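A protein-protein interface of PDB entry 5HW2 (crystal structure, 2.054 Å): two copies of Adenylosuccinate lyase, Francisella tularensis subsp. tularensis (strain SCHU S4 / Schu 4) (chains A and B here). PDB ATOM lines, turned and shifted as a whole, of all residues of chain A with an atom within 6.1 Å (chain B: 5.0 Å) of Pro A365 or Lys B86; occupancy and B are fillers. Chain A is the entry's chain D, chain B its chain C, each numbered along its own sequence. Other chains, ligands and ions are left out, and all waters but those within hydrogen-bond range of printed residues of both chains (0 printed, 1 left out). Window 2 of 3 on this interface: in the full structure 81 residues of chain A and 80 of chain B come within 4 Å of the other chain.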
ATOM      1  N   LEU A 360      18.244  31.367 -35.973  1.00  0.00           N
ATOM      2  CA  LEU A 360      19.070  31.510 -34.780  1.00  0.00           C
ATOM      3  C   LEU A 360      18.515  30.711 -33.608  1.00  0.00           C
ATOM      4  O   LEU A 360      19.281  30.270 -32.746  1.00  0.00           O
ATOM      5  CB  LEU A 360      19.202  32.985 -34.401  1.00  0.00           C
ATOM      6  CG  LEU A 360      19.979  33.862 -35.386  1.00  0.00           C
ATOM      7  CD1 LEU A 360      20.176  35.263 -34.827  1.00  0.00           C
ATOM      8  CD2 LEU A 360      21.317  33.225 -35.726  1.00  0.00           C
ATOM      9  N   VAL A 361      17.196  30.516 -33.553  1.00  0.00           N
ATOM     10  CA  VAL A 361      16.624  29.687 -32.497  1.00  0.00           C
ATOM     11  C   VAL A 361      16.984  28.222 -32.716  1.00  0.00           C
ATOM     12  O   VAL A 361      17.295  27.495 -31.765  1.00  0.00           O
ATOM     13  CB  VAL A 361      15.100  29.897 -32.422  1.00  0.00           C
ATOM     14  CG1 VAL A 361      14.456  28.834 -31.546  1.00  0.00           C
ATOM     15  CG2 VAL A 361      14.783  31.282 -31.883  1.00  0.00           C
ATOM     16  N   ALA A 362      16.971  27.773 -33.972  1.00  0.00           N
ATOM     17  CA  ALA A 362      17.219  26.364 -34.264  1.00  0.00           C
ATOM     18  C   ALA A 362      18.689  25.996 -34.102  1.00  0.00           C
ATOM     19  O   ALA A 362      19.006  24.932 -33.559  1.00  0.00           O
ATOM     20  CB  ALA A 362      16.744  26.033 -35.679  1.00  0.00           C
ATOM     21  N   ASN A 363      19.599  26.855 -34.561  1.00  0.00           N
ATOM     22  CA  ASN A 363      21.011  26.508 -34.632  1.00  0.00           C
ATOM     23  C   ASN A 363      21.841  27.072 -33.485  1.00  0.00           C
ATOM     24  O   ASN A 363      23.021  26.723 -33.372  1.00  0.00           O
ATOM     25  CB  ASN A 363      21.597  26.978 -35.969  1.00  0.00           C
ATOM     26  CG  ASN A 363      20.683  26.673 -37.139  1.00  0.00           C
ATOM     27  OD1 ASN A 363      20.434  27.527 -37.986  1.00  0.00           O
ATOM     28  ND2 ASN A 363      20.170  25.448 -37.187  1.00  0.00           N
ATOM     29  N   THR A 364      21.267  27.926 -32.642  1.00  0.00           N
ATOM     30  CA  THR A 364      21.967  28.424 -31.469  1.00  0.00           C
ATOM     31  C   THR A 364      21.174  28.093 -30.211  1.00  0.00           C
ATOM     32  O   THR A 364      19.940  28.041 -30.244  1.00  0.00           O
ATOM     33  CB  THR A 364      22.190  29.940 -31.533  1.00  0.00           C
ATOM     34  OG1 THR A 364      20.947  30.617 -31.307  1.00  0.00           O
ATOM     35  CG2 THR A 364      22.735  30.345 -32.889  1.00  0.00           C
ATOM     36  N   PRO A 365      21.853  27.863 -29.084  1.00  0.00           N
ATOM     37  CA  PRO A 365      21.133  27.601 -27.830  1.00  0.00           C
ATOM     38  C   PRO A 365      20.654  28.874 -27.147  1.00  0.00           C
ATOM     39  O   PRO A 365      20.789  29.018 -25.927  1.00  0.00           O
ATOM     40  CB  PRO A 365      22.176  26.867 -26.982  1.00  0.00           C
ATOM     41  CG  PRO A 365      23.478  27.418 -27.460  1.00  0.00           C
ATOM     42  CD  PRO A 365      23.308  27.681 -28.936  1.00  0.00           C
ATOM     43  N   PHE A 366      20.095  29.801 -27.918  1.00  0.00           N
ATOM     44  CA  PHE A 366      19.572  31.053 -27.396  1.00  0.00           C
ATOM     45  C   PHE A 366      18.050  31.050 -27.449  1.00  0.00           C
ATOM     46  O   PHE A 366      17.443  30.394 -28.300  1.00  0.00           O
ATOM     47  CB  PHE A 366      20.109  32.254 -28.181  1.00  0.00           C
ATOM     48  CG  PHE A 366      21.534  32.603 -27.863  1.00  0.00           C
ATOM     49  CD1 PHE A 366      22.249  31.883 -26.921  1.00  0.00           C
ATOM     50  CD2 PHE A 366      22.157  33.664 -28.501  1.00  0.00           C
ATOM     51  CE1 PHE A 366      23.561  32.207 -26.628  1.00  0.00           C
ATOM     52  CE2 PHE A 366      23.468  33.995 -28.212  1.00  0.00           C
ATOM     53  CZ  PHE A 366      24.169  33.265 -27.275  1.00  0.00           C
ATOM     54  N   MET A 367      17.442  31.799 -26.536  1.00  0.00           N
ATOM     55  CA  MET A 367      15.992  31.878 -26.464  1.00  0.00           C
ATOM     56  C   MET A 367      15.451  32.810 -27.547  1.00  0.00           C
ATOM     57  O   MET A 367      16.201  33.473 -28.270  1.00  0.00           O
ATOM     58  CB  MET A 367      15.555  32.345 -25.077  1.00  0.00           C
ATOM     59  CG  MET A 367      16.191  31.559 -23.941  1.00  0.00           C
ATOM     60  SD  MET A 367      15.992  29.775 -24.128  1.00  0.00           S
ATOM     61  CE  MET A 367      16.981  29.177 -22.761  1.00  0.00           C
ATOM     62  N   ARG A 368      14.120  32.854 -27.652  1.00  0.00           N
ATOM     63  CA  ARG A 368      13.477  33.640 -28.702  1.00  0.00           C
ATOM     64  C   ARG A 368      13.789  35.124 -28.557  1.00  0.00           C
ATOM     65  O   ARG A 368      14.253  35.767 -29.505  1.00  0.00           O
ATOM     66  CB  ARG A 368      11.966  33.408 -28.683  1.00  0.00           C
ATOM     67  CG  ARG A 368      11.501  32.217 -29.503  1.00  0.00           C
ATOM     68  CD  ARG A 368       9.991  32.232 -29.679  1.00  0.00           C
ATOM     69  NE  ARG A 368       9.528  31.159 -30.554  1.00  0.00           N
ATOM     70  CZ  ARG A 368       9.384  31.279 -31.872  1.00  0.00           C
ATOM     71  NH1 ARG A 368       9.669  32.427 -32.470  1.00  0.00           N
ATOM     72  NH2 ARG A 368       8.955  30.250 -32.589  1.00  0.00           N
ATOM     73  N   THR B  81      10.456  25.838 -18.124  1.00  0.00           N
ATOM     74  CA  THR B  81      11.649  26.661 -18.201  1.00  0.00           C
ATOM     75  C   THR B  81      11.733  27.344 -19.562  1.00  0.00           C
ATOM     76  O   THR B  81      11.053  26.967 -20.521  1.00  0.00           O
ATOM     77  CB  THR B  81      12.905  25.823 -17.967  1.00  0.00           C
ATOM     78  OG1 THR B  81      13.271  25.156 -19.182  1.00  0.00           O
ATOM     79  CG2 THR B  81      12.653  24.783 -16.885  1.00  0.00           C
ATOM     80  N   ALA B  82      12.586  28.369 -19.636  1.00  0.00           N
ATOM     81  CA  ALA B  82      12.801  29.052 -20.906  1.00  0.00           C
ATOM     82  C   ALA B  82      13.396  28.116 -21.947  1.00  0.00           C
ATOM     83  O   ALA B  82      13.138  28.277 -23.146  1.00  0.00           O
ATOM     84  CB  ALA B  82      13.704  30.269 -20.705  1.00  0.00           C
ATOM     85  N   GLU B  83      14.186  27.132 -21.509  1.00  0.00           N
ATOM     86  CA  GLU B  83      14.770  26.167 -22.435  1.00  0.00           C
ATOM     87  C   GLU B  83      13.785  25.057 -22.786  1.00  0.00           C
ATOM     88  O   GLU B  83      13.695  24.649 -23.950  1.00  0.00           O
ATOM     89  CB  GLU B  83      16.043  25.575 -21.830  1.00  0.00           C
ATOM     90  CG  GLU B  83      16.514  24.317 -22.447  1.00  0.00           C
ATOM     91  CD  GLU B  83      17.031  24.470 -23.818  1.00  0.00           C
ATOM     92  OE1 GLU B  83      17.532  25.435 -24.136  1.00  0.00           O
ATOM     93  OE2 GLU B  83      16.938  23.628 -24.592  1.00  0.00           O
ATOM     94  N   THR B  84      13.021  24.569 -21.804  1.00  0.00           N
ATOM     95  CA  THR B  84      12.098  23.468 -22.062  1.00  0.00           C
ATOM     96  C   THR B  84      11.010  23.876 -23.047  1.00  0.00           C
ATOM     97  O   THR B  84      10.599  23.077 -23.896  1.00  0.00           O
ATOM     98  CB  THR B  84      11.479  22.982 -20.750  1.00  0.00           C
ATOM     99  OG1 THR B  84      12.519  22.711 -19.802  1.00  0.00           O
ATOM    100  CG2 THR B  84      10.669  21.714 -20.976  1.00  0.00           C
ATOM    101  N   GLY B  85      10.535  25.115 -22.955  1.00  0.00           N
ATOM    102  CA  GLY B  85       9.517  25.598 -23.866  1.00  0.00           C
ATOM    103  C   GLY B  85      10.082  26.446 -24.986  1.00  0.00           C
ATOM    104  O   GLY B  85       9.364  27.247 -25.591  1.00  0.00           O
ATOM    105  N   LYS B  86      11.374  26.274 -25.271  1.00  0.00           N
ATOM    106  CA  LYS B  86      12.025  27.077 -26.302  1.00  0.00           C
ATOM    107  C   LYS B  86      11.476  26.753 -27.687  1.00  0.00           C
ATOM    108  O   LYS B  86      11.152  27.658 -28.466  1.00  0.00           O
ATOM    109  CB  LYS B  86      13.537  26.859 -26.255  1.00  0.00           C
ATOM    110  CG  LYS B  86      14.289  27.425 -27.443  1.00  0.00           C
ATOM    111  CD  LYS B  86      15.755  27.027 -27.398  1.00  0.00           C
ATOM    112  CE  LYS B  86      16.471  27.416 -28.678  1.00  0.00           C
ATOM    113  NZ  LYS B  86      17.915  27.058 -28.643  1.00  0.00           N
ATOM    114  N   PHE B  87      11.364  25.467 -28.012  1.00  0.00           N
ATOM    115  CA  PHE B  87      10.894  25.030 -29.319  1.00  0.00           C
ATOM    116  C   PHE B  87       9.385  24.834 -29.373  1.00  0.00           C
ATOM    117  O   PHE B  87       8.886  24.218 -30.322  1.00  0.00           O
ATOM    118  CB  PHE B  87      11.603  23.737 -29.726  1.00  0.00           C
ATOM    119  CG  PHE B  87      13.083  23.897 -29.923  1.00  0.00           C
ATOM    120  CD1 PHE B  87      13.589  24.355 -31.128  1.00  0.00           C
ATOM    121  CD2 PHE B  87      13.967  23.595 -28.901  1.00  0.00           C
ATOM    122  CE1 PHE B  87      14.950  24.506 -31.312  1.00  0.00           C
ATOM    123  CE2 PHE B  87      15.329  23.745 -29.078  1.00  0.00           C
ATOM    124  CZ  PHE B  87      15.820  24.201 -30.286  1.00  0.00           C
ATOM    125  N   PHE B  88       8.652  25.334 -28.385  1.00  0.00           N
ATOM    126  CA  PHE B  88       7.199  25.263 -28.427  1.00  0.00           C
ATOM    127  C   PHE B  88       6.660  26.241 -29.463  1.00  0.00           C
ATOM    128  O   PHE B  88       7.121  27.383 -29.559  1.00  0.00           O
ATOM    129  CB  PHE B  88       6.615  25.572 -27.049  1.00  0.00           C
ATOM    130  CG  PHE B  88       5.121  25.445 -26.980  1.00  0.00           C
ATOM    131  CD1 PHE B  88       4.525  24.203 -26.830  1.00  0.00           C
ATOM    132  CD2 PHE B  88       4.312  26.567 -27.057  1.00  0.00           C
ATOM    133  CE1 PHE B  88       3.150  24.082 -26.762  1.00  0.00           C
ATOM    134  CE2 PHE B  88       2.937  26.453 -26.990  1.00  0.00           C
ATOM    135  CZ  PHE B  88       2.354  25.209 -26.843  1.00  0.00           C
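Of the 9 printed residues of chain A, 5 touch a printed residue of chain B.
Printed residues of chain A that touch a printed residue of chain B: Val A361, Thr A364, Pro A365, Phe A366 and Met A367.
Hydrophobic or aromatic side chains of chain A within 4 Å of the printed part of chain B: Val A361 and Met A367.
Among the printed residues, no Asp or Glu carboxylate lies within 4 Å of a Lys or Arg side-chain nitrogen of the other chain.
OG1 of Thr B81 lies close to N of Glu B83 (3.2 Å).
Printed residues of chain B within 4 Å of Val A361: Lys B86 and Phe B87.
Of chain B, only Lys B86 comes within 4 Å of Pro A365.
Printed residues of chain B within 4 Å of Phe A366: Lys B86 (3.2 Å).
Of the printed residues of chain B, Met A367 touches Ala B82 (3.4 Å) and Glu B83 (3.7 Å).
Printed residues of chain A within 4 Å of Ala B82: Met A367 (3.4 Å).
Of chain A, only Val A361, Thr A364, Pro A365 and Phe A366 come within 4 Å of Lys B86.
Of the printed residues of chain A, Phe B87 touches Val A361 (3.8 Å).
The nearest printed residue of chain B that does not touch Pro A365 is Glu B83 (5.2 Å).
The backbone carbonyl oxygen of Thr A364 lies within hydrogen-bond range of the side-chain amino group of Lys B86, 2.8 Å away.
The backbone carbonyl oxygen (O) of Val A361 sits close to the side-chain amino group (NZ) of Lys B86 (3.2 Å).
The backbone carbonyl oxygen (O) of Phe A366 lies close to the side-chain amino group (NZ) of Lys B86, at 3.4 Å.
The backbone carbonyl oxygen of Ala B82 lies close to the side-chain sulfur of Met A367, 3.4 Å away.
Phe B87 touches Val A361 (CE1 to O, 3.8 Å).
Lys B86 touches Pro A365.
Glu B83 touches Met A367 (N to CE, 3.7 Å).
No position is printed for both chains.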
